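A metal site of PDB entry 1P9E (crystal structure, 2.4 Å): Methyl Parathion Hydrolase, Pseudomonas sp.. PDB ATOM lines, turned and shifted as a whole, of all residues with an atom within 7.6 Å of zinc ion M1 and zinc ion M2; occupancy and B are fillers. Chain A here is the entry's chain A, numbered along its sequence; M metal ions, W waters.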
ATOM      1  N   LEU A  67     -24.651   0.962  -4.472  1.00  0.00           N
ATOM      2  CA  LEU A  67     -23.262   0.697  -4.809  1.00  0.00           C
ATOM      3  C   LEU A  67     -22.319   0.856  -3.618  1.00  0.00           C
ATOM      4  O   LEU A  67     -22.508   1.730  -2.768  1.00  0.00           O
ATOM      5  CB  LEU A  67     -22.808   1.650  -5.925  1.00  0.00           C
ATOM      6  CG  LEU A  67     -23.637   1.563  -7.210  1.00  0.00           C
ATOM      7  CD1 LEU A  67     -23.200   2.670  -8.186  1.00  0.00           C
ATOM      8  CD2 LEU A  67     -23.495   0.168  -7.821  1.00  0.00           C
ATOM      9  N   SER A  96     -28.535   6.855  -8.529  1.00  0.00           N
ATOM     10  CA  SER A  96     -29.432   6.943  -9.657  1.00  0.00           C
ATOM     11  C   SER A  96     -28.639   6.664 -10.943  1.00  0.00           C
ATOM     12  O   SER A  96     -27.419   6.877 -10.990  1.00  0.00           O
ATOM     13  CB  SER A  96     -30.109   8.322  -9.689  1.00  0.00           C
ATOM     14  OG  SER A  96     -29.146   9.340  -9.877  1.00  0.00           O
ATOM     15  N   VAL A  97     -29.330   6.153 -11.954  1.00  0.00           N
ATOM     16  CA  VAL A  97     -28.731   5.836 -13.251  1.00  0.00           C
ATOM     17  C   VAL A  97     -29.583   6.639 -14.222  1.00  0.00           C
ATOM     18  O   VAL A  97     -30.784   6.384 -14.336  1.00  0.00           O
ATOM     19  CB  VAL A  97     -28.848   4.344 -13.561  1.00  0.00           C
ATOM     20  CG1 VAL A  97     -28.364   4.065 -14.974  1.00  0.00           C
ATOM     21  CG2 VAL A  97     -28.043   3.539 -12.534  1.00  0.00           C
ATOM     22  N   THR A  98     -28.965   7.594 -14.918  1.00  0.00           N
ATOM     23  CA  THR A  98     -29.721   8.484 -15.795  1.00  0.00           C
ATOM     24  C   THR A  98     -29.282   8.680 -17.257  1.00  0.00           C
ATOM     25  O   THR A  98     -28.099   8.555 -17.608  1.00  0.00           O
ATOM     26  CB  THR A  98     -29.792   9.866 -15.102  1.00  0.00           C
ATOM     27  OG1 THR A  98     -30.179   9.677 -13.729  1.00  0.00           O
ATOM     28  CG2 THR A  98     -30.822  10.766 -15.767  1.00  0.00           C
ATOM     29  N   ASP A 112     -27.273   8.215 -23.780  1.00  0.00           N
ATOM     30  CA  ASP A 112     -27.204   7.050 -22.920  1.00  0.00           C
ATOM     31  C   ASP A 112     -28.595   6.457 -22.834  1.00  0.00           C
ATOM     32  O   ASP A 112     -29.602   7.176 -22.938  1.00  0.00           O
ATOM     33  CB  ASP A 112     -26.601   7.431 -21.568  1.00  0.00           C
ATOM     34  CG  ASP A 112     -25.070   7.562 -21.652  1.00  0.00           C
ATOM     35  OD1 ASP A 112     -24.422   7.914 -20.651  1.00  0.00           O
ATOM     36  OD2 ASP A 112     -24.516   7.312 -22.759  1.00  0.00           O
ATOM     37  N   THR A 146     -22.028   7.943 -24.014  1.00  0.00           N
ATOM     38  CA  THR A 146     -20.891   8.563 -23.339  1.00  0.00           C
ATOM     39  C   THR A 146     -19.807   7.470 -23.291  1.00  0.00           C
ATOM     40  O   THR A 146     -18.647   7.708 -23.642  1.00  0.00           O
ATOM     41  CB  THR A 146     -21.257   9.039 -21.891  1.00  0.00           C
ATOM     42  OG1 THR A 146     -21.838   7.966 -21.150  1.00  0.00           O
ATOM     43  CG2 THR A 146     -22.265  10.188 -21.948  1.00  0.00           C
ATOM     44  N   HIS A 147     -20.191   6.270 -22.850  1.00  0.00           N
ATOM     45  CA  HIS A 147     -19.269   5.147 -22.788  1.00  0.00           C
ATOM     46  C   HIS A 147     -20.082   3.862 -22.795  1.00  0.00           C
ATOM     47  O   HIS A 147     -21.292   3.879 -22.493  1.00  0.00           O
ATOM     48  CB  HIS A 147     -18.337   5.219 -21.563  1.00  0.00           C
ATOM     49  CG  HIS A 147     -19.049   5.212 -20.250  1.00  0.00           C
ATOM     50  ND1 HIS A 147     -19.961   6.175 -19.881  1.00  0.00           N
ATOM     51  CD2 HIS A 147     -18.963   4.354 -19.189  1.00  0.00           C
ATOM     52  CE1 HIS A 147     -20.398   5.924 -18.656  1.00  0.00           C
ATOM     53  NE2 HIS A 147     -19.805   4.832 -18.218  1.00  0.00           N
ATOM     54  N   MET A 148     -19.440   2.756 -23.143  1.00  0.00           N
ATOM     55  CA  MET A 148     -20.157   1.485 -23.244  1.00  0.00           C
ATOM     56  C   MET A 148     -20.274   0.595 -22.023  1.00  0.00           C
ATOM     57  O   MET A 148     -20.151  -0.625 -22.142  1.00  0.00           O
ATOM     58  CB  MET A 148     -19.580   0.672 -24.400  1.00  0.00           C
ATOM     59  CG  MET A 148     -19.834   1.306 -25.756  1.00  0.00           C
ATOM     60  SD  MET A 148     -19.147   0.333 -27.096  1.00  0.00           S
ATOM     61  CE  MET A 148     -18.965   1.636 -28.406  1.00  0.00           C
ATOM     62  N   HIS A 149     -20.512   1.178 -20.857  1.00  0.00           N
ATOM     63  CA  HIS A 149     -20.710   0.351 -19.685  1.00  0.00           C
ATOM     64  C   HIS A 149     -22.116  -0.213 -19.751  1.00  0.00           C
ATOM     65  O   HIS A 149     -22.979   0.328 -20.449  1.00  0.00           O
ATOM     66  CB  HIS A 149     -20.488   1.158 -18.414  1.00  0.00           C
ATOM     67  CG  HIS A 149     -19.083   1.101 -17.917  1.00  0.00           C
ATOM     68  ND1 HIS A 149     -18.619   1.891 -16.882  1.00  0.00           N
ATOM     69  CD2 HIS A 149     -18.037   0.321 -18.292  1.00  0.00           C
ATOM     70  CE1 HIS A 149     -17.344   1.606 -16.657  1.00  0.00           C
ATOM     71  NE2 HIS A 149     -16.973   0.659 -17.495  1.00  0.00           N
ATOM     72  N   PRO A 150     -22.373  -1.291 -19.011  1.00  0.00           N
ATOM     73  CA  PRO A 150     -23.700  -1.919 -19.012  1.00  0.00           C
ATOM     74  C   PRO A 150     -24.842  -0.937 -18.765  1.00  0.00           C
ATOM     75  O   PRO A 150     -25.866  -0.985 -19.459  1.00  0.00           O
ATOM     76  CB  PRO A 150     -23.598  -2.962 -17.894  1.00  0.00           C
ATOM     77  CG  PRO A 150     -22.126  -3.205 -17.752  1.00  0.00           C
ATOM     78  CD  PRO A 150     -21.519  -1.848 -17.938  1.00  0.00           C
ATOM     79  N   ASP A 151     -24.659  -0.062 -17.782  1.00  0.00           N
ATOM     80  CA  ASP A 151     -25.690   0.902 -17.398  1.00  0.00           C
ATOM     81  C   ASP A 151     -25.822   2.116 -18.334  1.00  0.00           C
ATOM     82  O   ASP A 151     -26.453   3.124 -17.997  1.00  0.00           O
ATOM     83  CB  ASP A 151     -25.466   1.361 -15.952  1.00  0.00           C
ATOM     84  CG  ASP A 151     -24.090   1.969 -15.744  1.00  0.00           C
ATOM     85  OD1 ASP A 151     -23.086   1.336 -16.167  1.00  0.00           O
ATOM     86  OD2 ASP A 151     -24.020   3.085 -15.159  1.00  0.00           O
ATOM     87  N   HIS A 152     -25.224   2.011 -19.522  1.00  0.00           N
ATOM     88  CA  HIS A 152     -25.338   3.083 -20.478  1.00  0.00           C
ATOM     89  C   HIS A 152     -25.749   2.530 -21.828  1.00  0.00           C
ATOM     90  O   HIS A 152     -26.426   3.212 -22.599  1.00  0.00           O
ATOM     91  CB  HIS A 152     -24.020   3.845 -20.551  1.00  0.00           C
ATOM     92  CG  HIS A 152     -23.661   4.540 -19.275  1.00  0.00           C
ATOM     93  ND1 HIS A 152     -23.876   5.884 -19.080  1.00  0.00           N
ATOM     94  CD2 HIS A 152     -23.180   4.055 -18.101  1.00  0.00           C
ATOM     95  CE1 HIS A 152     -23.552   6.203 -17.840  1.00  0.00           C
ATOM     96  NE2 HIS A 152     -23.121   5.116 -17.218  1.00  0.00           N
ATOM     97  N   TRP A 179     -14.266  -2.114 -26.557  1.00  0.00           N
ATOM     98  CA  TRP A 179     -15.316  -3.018 -26.087  1.00  0.00           C
ATOM     99  C   TRP A 179     -15.809  -4.080 -27.079  1.00  0.00           C
ATOM    100  O   TRP A 179     -16.174  -5.189 -26.676  1.00  0.00           O
ATOM    101  CB  TRP A 179     -16.537  -2.205 -25.604  1.00  0.00           C
ATOM    102  CG  TRP A 179     -16.250  -1.394 -24.374  1.00  0.00           C
ATOM    103  CD1 TRP A 179     -16.143  -0.037 -24.290  1.00  0.00           C
ATOM    104  CD2 TRP A 179     -16.047  -1.902 -23.058  1.00  0.00           C
ATOM    105  NE1 TRP A 179     -15.875   0.338 -23.000  1.00  0.00           N
ATOM    106  CE2 TRP A 179     -15.813  -0.788 -22.214  1.00  0.00           C
ATOM    107  CE3 TRP A 179     -16.046  -3.182 -22.498  1.00  0.00           C
ATOM    108  CZ2 TRP A 179     -15.572  -0.926 -20.839  1.00  0.00           C
ATOM    109  CZ3 TRP A 179     -15.797  -3.316 -21.127  1.00  0.00           C
ATOM    110  CH2 TRP A 179     -15.564  -2.185 -20.316  1.00  0.00           C
ATOM    111  N   PHE A 196     -18.983  -7.426 -19.313  1.00  0.00           N
ATOM    112  CA  PHE A 196     -19.015  -6.054 -19.785  1.00  0.00           C
ATOM    113  C   PHE A 196     -18.760  -6.082 -21.292  1.00  0.00           C
ATOM    114  O   PHE A 196     -19.476  -5.438 -22.056  1.00  0.00           O
ATOM    115  CB  PHE A 196     -17.936  -5.217 -19.088  1.00  0.00           C
ATOM    116  CG  PHE A 196     -18.332  -4.755 -17.718  1.00  0.00           C
ATOM    117  CD1 PHE A 196     -18.763  -5.659 -16.757  1.00  0.00           C
ATOM    118  CD2 PHE A 196     -18.281  -3.402 -17.397  1.00  0.00           C
ATOM    119  CE1 PHE A 196     -19.135  -5.237 -15.489  1.00  0.00           C
ATOM    120  CE2 PHE A 196     -18.660  -2.968 -16.128  1.00  0.00           C
ATOM    121  CZ  PHE A 196     -19.099  -3.884 -15.170  1.00  0.00           C
ATOM    122  N   HIS A 234     -12.293   7.596 -17.889  1.00  0.00           N
ATOM    123  CA  HIS A 234     -13.174   6.663 -17.203  1.00  0.00           C
ATOM    124  C   HIS A 234     -13.061   5.387 -18.023  1.00  0.00           C
ATOM    125  O   HIS A 234     -13.005   4.281 -17.483  1.00  0.00           O
ATOM    126  CB  HIS A 234     -14.632   7.164 -17.180  1.00  0.00           C
ATOM    127  CG  HIS A 234     -15.599   6.211 -16.541  1.00  0.00           C
ATOM    128  ND1 HIS A 234     -15.454   5.745 -15.249  1.00  0.00           N
ATOM    129  CD2 HIS A 234     -16.732   5.619 -17.023  1.00  0.00           C
ATOM    130  CE1 HIS A 234     -16.447   4.916 -14.960  1.00  0.00           C
ATOM    131  NE2 HIS A 234     -17.237   4.819 -16.021  1.00  0.00           N
ATOM    132  N   THR A 235     -13.043   5.572 -19.344  1.00  0.00           N
ATOM    133  CA  THR A 235     -12.887   4.475 -20.311  1.00  0.00           C
ATOM    134  C   THR A 235     -12.059   5.074 -21.457  1.00  0.00           C
ATOM    135  O   THR A 235     -11.972   6.307 -21.582  1.00  0.00           O
ATOM    136  CB  THR A 235     -14.238   3.929 -20.808  1.00  0.00           C
ATOM    137  OG1 THR A 235     -14.981   4.986 -21.420  1.00  0.00           O
ATOM    138  CG2 THR A 235     -15.038   3.352 -19.655  1.00  0.00           C
ATOM    139  N   HIS A 238     -14.304   7.596 -23.440  1.00  0.00           N
ATOM    140  CA  HIS A 238     -15.409   8.239 -22.726  1.00  0.00           C
ATOM    141  C   HIS A 238     -15.649   9.587 -23.375  1.00  0.00           C
ATOM    142  O   HIS A 238     -14.706  10.341 -23.647  1.00  0.00           O
ATOM    143  CB  HIS A 238     -15.087   8.404 -21.228  1.00  0.00           C
ATOM    144  CG  HIS A 238     -16.213   9.010 -20.446  1.00  0.00           C
ATOM    145  ND1 HIS A 238     -16.272  10.337 -20.124  1.00  0.00           N
ATOM    146  CD2 HIS A 238     -17.356   8.449 -19.961  1.00  0.00           C
ATOM    147  CE1 HIS A 238     -17.394  10.590 -19.475  1.00  0.00           C
ATOM    148  NE2 HIS A 238     -18.075   9.459 -19.368  1.00  0.00           N
ATOM    149  N   GLY A 254     -21.697  12.212 -18.634  1.00  0.00           N
ATOM    150  CA  GLY A 254     -21.568  10.773 -18.525  1.00  0.00           C
ATOM    151  C   GLY A 254     -21.148  10.337 -17.114  1.00  0.00           C
ATOM    152  O   GLY A 254     -21.777  10.712 -16.123  1.00  0.00           O
ATOM    153  N   ASP A 255     -20.094   9.531 -17.012  1.00  0.00           N
ATOM    154  CA  ASP A 255     -19.612   9.059 -15.718  1.00  0.00           C
ATOM    155  C   ASP A 255     -18.318   9.837 -15.409  1.00  0.00           C
ATOM    156  O   ASP A 255     -17.424   9.328 -14.713  1.00  0.00           O
ATOM    157  CB  ASP A 255     -19.320   7.535 -15.750  1.00  0.00           C
ATOM    158  CG  ASP A 255     -20.577   6.658 -15.604  1.00  0.00           C
ATOM    159  OD1 ASP A 255     -21.701   7.217 -15.590  1.00  0.00           O
ATOM    160  OD2 ASP A 255     -20.452   5.402 -15.503  1.00  0.00           O
ATOM    161  N   LEU A 256     -18.194  11.053 -15.914  1.00  0.00           N
ATOM    162  CA  LEU A 256     -16.973  11.818 -15.643  1.00  0.00           C
ATOM    163  C   LEU A 256     -16.798  12.001 -14.122  1.00  0.00           C
ATOM    164  O   LEU A 256     -15.675  12.194 -13.621  1.00  0.00           O
ATOM    165  CB  LEU A 256     -17.010  13.186 -16.335  1.00  0.00           C
ATOM    166  CG  LEU A 256     -15.734  13.602 -17.092  1.00  0.00           C
ATOM    167  CD1 LEU A 256     -15.708  15.123 -17.197  1.00  0.00           C
ATOM    168  CD2 LEU A 256     -14.494  13.107 -16.355  1.00  0.00           C
ATOM    169  N   ILE A 257     -17.933  11.956 -13.400  1.00  0.00           N
ATOM    170  CA  ILE A 257     -17.954  12.030 -11.945  1.00  0.00           C
ATOM    171  C   ILE A 257     -18.947  10.979 -11.472  1.00  0.00           C
ATOM    172  O   ILE A 257     -20.041  10.859 -12.034  1.00  0.00           O
ATOM    173  CB  ILE A 257     -18.351  13.428 -11.398  1.00  0.00           C
ATOM    174  CG1 ILE A 257     -18.614  13.316  -9.887  1.00  0.00           C
ATOM    175  CG2 ILE A 257     -19.561  13.970 -12.124  1.00  0.00           C
ATOM    176  CD1 ILE A 257     -18.571  14.619  -9.125  1.00  0.00           C
ATOM    177  N   LEU A 258     -18.553  10.213 -10.462  1.00  0.00           N
ATOM    178  CA  LEU A 258     -19.365   9.105  -9.932  1.00  0.00           C
ATOM    179  C   LEU A 258     -19.985   9.264  -8.523  1.00  0.00           C
ATOM    180  O   LEU A 258     -21.059   8.697  -8.263  1.00  0.00           O
ATOM    181  CB  LEU A 258     -18.520   7.823  -9.928  1.00  0.00           C
ATOM    182  CG  LEU A 258     -17.869   7.447 -11.258  1.00  0.00           C
ATOM    183  CD1 LEU A 258     -16.804   6.379 -11.045  1.00  0.00           C
ATOM    184  CD2 LEU A 258     -18.947   6.939 -12.228  1.00  0.00           C
ATOM    185  N   LEU A 273     -12.675   1.932 -10.913  1.00  0.00           N
ATOM    186  CA  LEU A 273     -13.510   1.702 -12.087  1.00  0.00           C
ATOM    187  C   LEU A 273     -13.013   2.496 -13.292  1.00  0.00           C
ATOM    188  O   LEU A 273     -13.477   2.276 -14.403  1.00  0.00           O
ATOM    189  CB  LEU A 273     -14.958   2.088 -11.787  1.00  0.00           C
ATOM    190  CG  LEU A 273     -15.551   1.316 -10.602  1.00  0.00           C
ATOM    191  CD1 LEU A 273     -16.720   2.064  -9.982  1.00  0.00           C
ATOM    192  CD2 LEU A 273     -15.973  -0.059 -11.106  1.00  0.00           C
ATOM    193  N   ASP A 274     -12.064   3.414 -13.058  1.00  0.00           N
ATOM    194  CA  ASP A 274     -11.511   4.257 -14.116  1.00  0.00           C
ATOM    195  C   ASP A 274     -10.298   3.638 -14.784  1.00  0.00           C
ATOM    196  O   ASP A 274      -9.469   3.015 -14.120  1.00  0.00           O
ATOM    197  CB  ASP A 274     -11.113   5.635 -13.558  1.00  0.00           C
ATOM    198  CG  ASP A 274     -12.286   6.366 -12.963  1.00  0.00           C
ATOM    199  OD1 ASP A 274     -13.202   6.761 -13.731  1.00  0.00           O
ATOM    200  OD2 ASP A 274     -12.291   6.558 -11.728  1.00  0.00           O
ATOM    201  N   SER A 301     -24.650  10.952 -15.202  1.00  0.00           N
ATOM    202  CA  SER A 301     -25.509   9.790 -15.037  1.00  0.00           C
ATOM    203  C   SER A 301     -25.767   9.339 -13.615  1.00  0.00           C
ATOM    204  O   SER A 301     -26.767   8.652 -13.363  1.00  0.00           O
ATOM    205  CB  SER A 301     -24.935   8.620 -15.830  1.00  0.00           C
ATOM    206  OG  SER A 301     -24.541   9.035 -17.137  1.00  0.00           O
ATOM    207  N   HIS A 302     -24.893   9.708 -12.665  1.00  0.00           N
ATOM    208  CA  HIS A 302     -25.079   9.233 -11.297  1.00  0.00           C
ATOM    209  C   HIS A 302     -25.220  10.253 -10.184  1.00  0.00           C
ATOM    210  O   HIS A 302     -25.056   9.890  -9.017  1.00  0.00           O
ATOM    211  CB  HIS A 302     -23.981   8.227 -10.970  1.00  0.00           C
ATOM    212  CG  HIS A 302     -23.917   7.099 -11.958  1.00  0.00           C
ATOM    213  ND1 HIS A 302     -24.962   6.225 -12.163  1.00  0.00           N
ATOM    214  CD2 HIS A 302     -22.971   6.761 -12.863  1.00  0.00           C
ATOM    215  CE1 HIS A 302     -24.659   5.399 -13.157  1.00  0.00           C
ATOM    216  NE2 HIS A 302     -23.458   5.710 -13.598  1.00  0.00           N
HETATM  217 ZN    ZN M   1     -22.509   4.628 -15.235  1.00  0.00          ZN
HETATM  218 ZN    ZN M   2     -19.022   3.794 -16.190  1.00  0.00          ZN
HETATM  219  O   HOH W   1     -18.644   3.210 -13.800  1.00  0.00           O
HETATM  220  O   HOH W   2     -20.980   3.102 -15.598  1.00  0.00           O
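The side-chain carboxylate of Asp 274 lies within hydrogen-bond range of a ring nitrogen (ND1) of His 234, at 2.9 Å.
ND1 of His 152 sits at hydrogen-bond distance from OD1 of Asp 112 (2.6 Å).
A ring nitrogen (ND1) of His 302 sits at hydrogen-bond distance from the backbone carbonyl oxygen (O) of Ser 96 (2.8 Å).
The backbone NH (N) of Asp 255 lies within hydrogen-bond range of a ring nitrogen (NE2) of His 238 (3.1 Å).
ND1 of His 147 lies within hydrogen-bond range of OG1 of Thr 146 (2.9 Å).
Within 4 Å of zinc ion M1: Asp 151, His 152, Asp 255 and His 302.
Of the 26 residues printed, 4 come within 4 Å of zinc ion M2.
A ring nitrogen (NE2) of His 152 binds zinc ion M1, 2.1 Å away.
OD2 of Asp 151 binds zinc ion M1 (2.2 Å).
NE2 of His 302 binds zinc ion M1 (2.2 Å).
Zinc ion M1 is bound by water W2, 2.2 Å away.
OD2 of Asp 255 is bound to zinc ion M1 (2.2 Å).
Slightly farther from zinc ion M1 lies OD1 of Asp 255 (2.7 Å).
Zinc ion M2 is bound by a ring nitrogen (ND1) of His 149 (2.1 Å), a ring nitrogen (NE2) of His 234 (2.1 Å), water W2 (2.2 Å), the side-chain carboxylate of Asp 255 (2.3 Å), a ring nitrogen (NE2) of His 147 (2.4 Å) and water W1 (2.5 Å).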
